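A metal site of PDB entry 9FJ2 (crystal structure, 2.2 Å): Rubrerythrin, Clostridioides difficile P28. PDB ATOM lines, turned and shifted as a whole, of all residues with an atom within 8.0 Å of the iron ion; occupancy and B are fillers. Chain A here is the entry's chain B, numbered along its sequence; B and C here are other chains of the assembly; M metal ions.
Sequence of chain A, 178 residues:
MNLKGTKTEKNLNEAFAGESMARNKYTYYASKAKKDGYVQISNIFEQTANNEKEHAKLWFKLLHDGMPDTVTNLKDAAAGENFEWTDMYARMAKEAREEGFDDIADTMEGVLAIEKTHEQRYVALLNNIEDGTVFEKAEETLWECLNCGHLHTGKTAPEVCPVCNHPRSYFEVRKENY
The side-chain sulfur (SG) of Cys 148 sits close to the backbone NH (N) of His 150 (3.5 Å). SG of Cys 145 lies close to N of Asn 147 (3.7 Å). N of Cys 161 sits at hydrogen-bond distance from O of His 166, at 2.9 Å. SG of Cys 161 sits close to N of Val 163 (3.5 Å). The backbone NH (N) of Cys 145 is in hydrogen-bond range of the backbone carbonyl oxygen (O) of His 150. The side-chain sulfur (SG) of Cys 164 sits close to the side-chain amide nitrogen (ND2) of Asn 147, at 3.4 Å. O of Cys 148 lies within hydrogen-bond range of NE2 of His 55 of chain C (2.8 Å).
Four residues have an atom within 4 Å of the iron ion: Cys 145, Cys 148, Cys 161 and Cys 164.
The iron ion is bound by SG of Cys 161, SG of Cys 164, SG of Cys 145 and SG of Cys 148.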
ATOM      1  N   GLU A 144      -5.995  13.452  10.005  1.00  0.00           N
ATOM      2  CA  GLU A 144      -4.897  13.499   9.046  1.00  0.00           C
ATOM      3  C   GLU A 144      -5.055  12.368   8.040  1.00  0.00           C
ATOM      4  O   GLU A 144      -5.325  11.228   8.427  1.00  0.00           O
ATOM      5  CB  GLU A 144      -3.545  13.389   9.757  1.00  0.00           C
ATOM      6  CG  GLU A 144      -2.345  13.499   8.836  1.00  0.00           C
ATOM      7  CD  GLU A 144      -1.027  13.270   9.557  1.00  0.00           C
ATOM      8  OE1 GLU A 144      -1.025  13.212  10.797  1.00  0.00           O
ATOM      9  OE2 GLU A 144       0.012  13.136   8.868  1.00  0.00           O
ATOM     10  N   CYS A 145      -4.887  12.691   6.768  1.00  0.00           N
ATOM     11  CA  CYS A 145      -4.925  11.692   5.701  1.00  0.00           C
ATOM     12  C   CYS A 145      -3.531  11.096   5.552  1.00  0.00           C
ATOM     13  O   CYS A 145      -2.591  11.801   5.161  1.00  0.00           O
ATOM     14  CB  CYS A 145      -5.414  12.314   4.389  1.00  0.00           C
ATOM     15  SG  CYS A 145      -5.541  11.143   3.016  1.00  0.00           S
ATOM     16  N   LEU A 146      -3.395   9.808   5.850  1.00  0.00           N
ATOM     17  CA  LEU A 146      -2.096   9.156   5.820  1.00  0.00           C
ATOM     18  C   LEU A 146      -1.556   8.974   4.408  1.00  0.00           C
ATOM     19  O   LEU A 146      -0.438   8.474   4.258  1.00  0.00           O
ATOM     20  CB  LEU A 146      -2.172   7.805   6.526  1.00  0.00           C
ATOM     21  CG  LEU A 146      -2.220   7.879   8.047  1.00  0.00           C
ATOM     22  CD1 LEU A 146      -2.338   6.488   8.651  1.00  0.00           C
ATOM     23  CD2 LEU A 146      -0.991   8.598   8.586  1.00  0.00           C
ATOM     24  N   ASN A 147      -2.302   9.369   3.371  1.00  0.00           N
ATOM     25  CA  ASN A 147      -1.845   9.253   1.992  1.00  0.00           C
ATOM     26  C   ASN A 147      -1.260  10.564   1.473  1.00  0.00           C
ATOM     27  O   ASN A 147      -0.101  10.597   1.048  1.00  0.00           O
ATOM     28  CB  ASN A 147      -2.999   8.796   1.093  1.00  0.00           C
ATOM     29  CG  ASN A 147      -2.536   8.368  -0.280  1.00  0.00           C
ATOM     30  OD1 ASN A 147      -1.727   7.452  -0.420  1.00  0.00           O
ATOM     31  ND2 ASN A 147      -3.038   9.040  -1.317  1.00  0.00           N
ATOM     32  N   CYS A 148      -2.039  11.639   1.509  1.00  0.00           N
ATOM     33  CA  CYS A 148      -1.606  12.933   0.990  1.00  0.00           C
ATOM     34  C   CYS A 148      -1.290  13.958   2.067  1.00  0.00           C
ATOM     35  O   CYS A 148      -0.559  14.910   1.786  1.00  0.00           O
ATOM     36  CB  CYS A 148      -2.675  13.516   0.052  1.00  0.00           C
ATOM     37  SG  CYS A 148      -4.167  14.098   0.896  1.00  0.00           S
ATOM     38  N   GLY A 149      -1.816  13.786   3.273  1.00  0.00           N
ATOM     39  CA  GLY A 149      -1.556  14.713   4.359  1.00  0.00           C
ATOM     40  C   GLY A 149      -2.630  15.737   4.622  1.00  0.00           C
ATOM     41  O   GLY A 149      -2.409  16.644   5.428  1.00  0.00           O
ATOM     42  N   HIS A 150      -3.786  15.619   3.979  1.00  0.00           N
ATOM     43  CA  HIS A 150      -4.856  16.595   4.162  1.00  0.00           C
ATOM     44  C   HIS A 150      -5.359  16.578   5.602  1.00  0.00           C
ATOM     45  O   HIS A 150      -5.576  15.509   6.190  1.00  0.00           O
ATOM     46  CB  HIS A 150      -6.009  16.312   3.199  1.00  0.00           C
ATOM     47  CG  HIS A 150      -7.257  17.072   3.503  1.00  0.00           C
ATOM     48  ND1 HIS A 150      -8.466  16.466   3.730  1.00  0.00           N
ATOM     49  CD2 HIS A 150      -7.480  18.407   3.624  1.00  0.00           C
ATOM     50  CE1 HIS A 150      -9.387  17.375   3.976  1.00  0.00           C
ATOM     51  NE2 HIS A 150      -8.815  18.565   3.915  1.00  0.00           N
ATOM     52  N   LEU A 151      -5.551  17.768   6.160  1.00  0.00           N
ATOM     53  CA  LEU A 151      -6.030  17.915   7.536  1.00  0.00           C
ATOM     54  C   LEU A 151      -7.499  18.304   7.522  1.00  0.00           C
ATOM     55  O   LEU A 151      -7.911  19.196   6.762  1.00  0.00           O
ATOM     56  CB  LEU A 151      -5.209  18.956   8.286  1.00  0.00           C
ATOM     57  CG  LEU A 151      -3.752  18.600   8.600  1.00  0.00           C
ATOM     58  CD1 LEU A 151      -3.230  19.420   9.770  1.00  0.00           C
ATOM     59  CD2 LEU A 151      -3.600  17.118   8.872  1.00  0.00           C
ATOM     60  N   VAL A 160     -14.701  10.498   2.140  1.00  0.00           N
ATOM     61  CA  VAL A 160     -13.658  10.399   1.119  1.00  0.00           C
ATOM     62  C   VAL A 160     -12.767  11.623   1.251  1.00  0.00           C
ATOM     63  O   VAL A 160     -13.272  12.753   1.380  1.00  0.00           O
ATOM     64  CB  VAL A 160     -14.254  10.308  -0.302  1.00  0.00           C
ATOM     65  CG1 VAL A 160     -13.194  10.608  -1.340  1.00  0.00           C
ATOM     66  CG2 VAL A 160     -14.858   8.936  -0.531  1.00  0.00           C
ATOM     67  N   CYS A 161     -11.461  11.415   1.227  1.00  0.00           N
ATOM     68  CA  CYS A 161     -10.533  12.527   1.257  1.00  0.00           C
ATOM     69  C   CYS A 161     -10.779  13.417   0.044  1.00  0.00           C
ATOM     70  O   CYS A 161     -10.834  12.924  -1.090  1.00  0.00           O
ATOM     71  CB  CYS A 161      -9.085  12.027   1.253  1.00  0.00           C
ATOM     72  SG  CYS A 161      -7.847  13.326   1.113  1.00  0.00           S
ATOM     73  N   PRO A 162     -10.953  14.729   0.232  1.00  0.00           N
ATOM     74  CA  PRO A 162     -11.244  15.618  -0.902  1.00  0.00           C
ATOM     75  C   PRO A 162     -10.012  16.053  -1.693  1.00  0.00           C
ATOM     76  O   PRO A 162     -10.160  16.873  -2.602  1.00  0.00           O
ATOM     77  CB  PRO A 162     -11.914  16.820  -0.228  1.00  0.00           C
ATOM     78  CG  PRO A 162     -11.647  16.693   1.259  1.00  0.00           C
ATOM     79  CD  PRO A 162     -10.819  15.465   1.493  1.00  0.00           C
ATOM     80  N   VAL A 163      -8.827  15.542  -1.372  1.00  0.00           N
ATOM     81  CA  VAL A 163      -7.610  15.916  -2.075  1.00  0.00           C
ATOM     82  C   VAL A 163      -7.159  14.747  -2.949  1.00  0.00           C
ATOM     83  O   VAL A 163      -7.147  14.846  -4.176  1.00  0.00           O
ATOM     84  CB  VAL A 163      -6.512  16.342  -1.098  1.00  0.00           C
ATOM     85  CG1 VAL A 163      -5.218  16.630  -1.844  1.00  0.00           C
ATOM     86  CG2 VAL A 163      -6.951  17.573  -0.302  1.00  0.00           C
ATOM     87  N   CYS A 164      -6.771  13.641  -2.319  1.00  0.00           N
ATOM     88  CA  CYS A 164      -6.296  12.467  -3.050  1.00  0.00           C
ATOM     89  C   CYS A 164      -7.415  11.484  -3.400  1.00  0.00           C
ATOM     90  O   CYS A 164      -7.149  10.517  -4.115  1.00  0.00           O
ATOM     91  CB  CYS A 164      -5.210  11.748  -2.243  1.00  0.00           C
ATOM     92  SG  CYS A 164      -5.768  11.041  -0.681  1.00  0.00           S
ATOM     93  N   ASN A 165      -8.632  11.711  -2.909  1.00  0.00           N
ATOM     94  CA  ASN A 165      -9.795  10.875  -3.218  1.00  0.00           C
ATOM     95  C   ASN A 165      -9.597   9.442  -2.756  1.00  0.00           C
ATOM     96  O   ASN A 165      -9.952   8.479  -3.451  1.00  0.00           O
ATOM     97  CB  ASN A 165     -10.131  10.932  -4.716  1.00  0.00           C
ATOM     98  CG  ASN A 165     -11.612  10.769  -4.992  1.00  0.00           C
ATOM     99  OD1 ASN A 165     -12.272   9.922  -4.383  1.00  0.00           O
ATOM    100  ND2 ASN A 165     -12.136  11.588  -5.891  1.00  0.00           N
ATOM    101  N   HIS A 166      -9.026   9.279  -1.559  1.00  0.00           N
ATOM    102  CA  HIS A 166      -8.897   7.989  -0.901  1.00  0.00           C
ATOM    103  C   HIS A 166      -9.946   7.846   0.201  1.00  0.00           C
ATOM    104  O   HIS A 166     -10.323   8.827   0.844  1.00  0.00           O
ATOM    105  CB  HIS A 166      -7.497   7.836  -0.296  1.00  0.00           C
ATOM    106  CG  HIS A 166      -6.437   7.498  -1.293  1.00  0.00           C
ATOM    107  ND1 HIS A 166      -5.535   6.474  -1.115  1.00  0.00           N
ATOM    108  CD2 HIS A 166      -6.139   8.046  -2.501  1.00  0.00           C
ATOM    109  CE1 HIS A 166      -4.725   6.407  -2.156  1.00  0.00           C
ATOM    110  NE2 HIS A 166      -5.068   7.348  -3.001  1.00  0.00           N
ATOM    111  N   PRO A 167     -10.444   6.623   0.441  1.00  0.00           N
ATOM    112  CA  PRO A 167     -11.564   6.454   1.383  1.00  0.00           C
ATOM    113  C   PRO A 167     -11.234   6.804   2.820  1.00  0.00           C
ATOM    114  O   PRO A 167     -10.087   7.139   3.147  1.00  0.00           O
ATOM    115  CB  PRO A 167     -11.915   4.966   1.234  1.00  0.00           C
ATOM    116  CG  PRO A 167     -10.674   4.333   0.714  1.00  0.00           C
ATOM    117  CD  PRO A 167     -10.037   5.352  -0.177  1.00  0.00           C
ATOM    118  N   TYR A 170      -7.986   5.841   5.385  1.00  0.00           N
ATOM    119  CA  TYR A 170      -6.660   6.438   5.463  1.00  0.00           C
ATOM    120  C   TYR A 170      -6.568   7.553   6.497  1.00  0.00           C
ATOM    121  O   TYR A 170      -5.532   8.224   6.560  1.00  0.00           O
ATOM    122  CB  TYR A 170      -6.254   6.986   4.084  1.00  0.00           C
ATOM    123  CG  TYR A 170      -5.768   5.918   3.125  1.00  0.00           C
ATOM    124  CD1 TYR A 170      -4.461   5.475   3.162  1.00  0.00           C
ATOM    125  CD2 TYR A 170      -6.627   5.370   2.180  1.00  0.00           C
ATOM    126  CE1 TYR A 170      -4.010   4.506   2.275  1.00  0.00           C
ATOM    127  CE2 TYR A 170      -6.189   4.402   1.299  1.00  0.00           C
ATOM    128  CZ  TYR A 170      -4.880   3.971   1.357  1.00  0.00           C
ATOM    129  OH  TYR A 170      -4.443   3.003   0.476  1.00  0.00           O
ATOM    130  N   PHE A 171      -7.604   7.770   7.299  1.00  0.00           N
ATOM    131  CA  PHE A 171      -7.656   8.905   8.212  1.00  0.00           C
ATOM    132  C   PHE A 171      -7.354   8.489   9.637  1.00  0.00           C
ATOM    133  O   PHE A 171      -7.736   7.397  10.078  1.00  0.00           O
ATOM    134  CB  PHE A 171      -9.031   9.587   8.139  1.00  0.00           C
ATOM    135  CG  PHE A 171      -9.130  10.597   7.032  1.00  0.00           C
ATOM    136  CD1 PHE A 171      -8.639  11.883   7.199  1.00  0.00           C
ATOM    137  CD2 PHE A 171      -9.723  10.266   5.817  1.00  0.00           C
ATOM    138  CE1 PHE A 171      -8.731  12.811   6.182  1.00  0.00           C
ATOM    139  CE2 PHE A 171      -9.815  11.194   4.799  1.00  0.00           C
ATOM    140  CZ  PHE A 171      -9.319  12.472   4.981  1.00  0.00           C
ATOM    141  N   ILE B 114      -1.852  21.670   2.497  1.00  0.00           N
ATOM    142  CA  ILE B 114      -0.979  20.623   3.016  1.00  0.00           C
ATOM    143  C   ILE B 114       0.456  21.118   3.101  1.00  0.00           C
ATOM    144  O   ILE B 114       1.154  20.859   4.089  1.00  0.00           O
ATOM    145  CB  ILE B 114      -1.095  19.355   2.144  1.00  0.00           C
ATOM    146  CG1 ILE B 114      -2.530  18.813   2.186  1.00  0.00           C
ATOM    147  CG2 ILE B 114      -0.100  18.299   2.609  1.00  0.00           C
ATOM    148  CD1 ILE B 114      -2.823  17.770   1.132  1.00  0.00           C
ATOM    149  N   ASN C  51       4.179  11.980   1.191  1.00  0.00           N
ATOM    150  CA  ASN C  51       3.078  12.905   0.903  1.00  0.00           C
ATOM    151  C   ASN C  51       3.278  13.582  -0.439  1.00  0.00           C
ATOM    152  O   ASN C  51       2.342  13.663  -1.249  1.00  0.00           O
ATOM    153  CB  ASN C  51       2.962  13.943   2.019  1.00  0.00           C
ATOM    154  CG  ASN C  51       2.198  13.432   3.214  1.00  0.00           C
ATOM    155  OD1 ASN C  51       1.666  12.334   3.204  1.00  0.00           O
ATOM    156  ND2 ASN C  51       2.146  14.251   4.273  1.00  0.00           N
ATOM    157  N   GLU C  54       2.476  11.428  -3.395  1.00  0.00           N
ATOM    158  CA  GLU C  54       1.065  11.298  -3.731  1.00  0.00           C
ATOM    159  C   GLU C  54       0.497  12.569  -4.361  1.00  0.00           C
ATOM    160  O   GLU C  54      -0.480  12.496  -5.116  1.00  0.00           O
ATOM    161  CB  GLU C  54       0.254  10.934  -2.486  1.00  0.00           C
ATOM    162  CG  GLU C  54       0.382   9.479  -2.062  1.00  0.00           C
ATOM    163  CD  GLU C  54      -0.172   8.523  -3.100  1.00  0.00           C
ATOM    164  OE1 GLU C  54      -1.300   8.754  -3.582  1.00  0.00           O
ATOM    165  OE2 GLU C  54       0.510   7.520  -3.418  1.00  0.00           O
ATOM    166  N   HIS C  55       1.090  13.736  -4.068  1.00  0.00           N
ATOM    167  CA  HIS C  55       0.641  14.962  -4.717  1.00  0.00           C
ATOM    168  C   HIS C  55       0.989  14.947  -6.201  1.00  0.00           C
ATOM    169  O   HIS C  55       0.176  15.365  -7.039  1.00  0.00           O
ATOM    170  CB  HIS C  55       1.261  16.180  -4.044  1.00  0.00           C
ATOM    171  CG  HIS C  55       0.906  16.332  -2.602  1.00  0.00           C
ATOM    172  ND1 HIS C  55       1.628  17.125  -1.736  1.00  0.00           N
ATOM    173  CD2 HIS C  55      -0.094  15.787  -1.861  1.00  0.00           C
ATOM    174  CE1 HIS C  55       1.087  17.064  -0.528  1.00  0.00           C
ATOM    175  NE2 HIS C  55       0.040  16.254  -0.580  1.00  0.00           N
ATOM    176  N   LEU C  58      -1.439  12.978  -8.380  1.00  0.00           N
ATOM    177  CA  LEU C  58      -2.654  13.681  -8.792  1.00  0.00           C
ATOM    178  C   LEU C  58      -2.437  14.432 -10.103  1.00  0.00           C
ATOM    179  O   LEU C  58      -3.256  14.349 -11.018  1.00  0.00           O
ATOM    180  CB  LEU C  58      -3.100  14.633  -7.692  1.00  0.00           C
ATOM    181  CG  LEU C  58      -3.379  14.001  -6.323  1.00  0.00           C
ATOM    182  CD1 LEU C  58      -3.827  15.052  -5.324  1.00  0.00           C
ATOM    183  CD2 LEU C  58      -4.419  12.901  -6.448  1.00  0.00           C
HETATM  184 FE    FE M   1      -5.745  12.444   1.136  1.00  0.00          FE
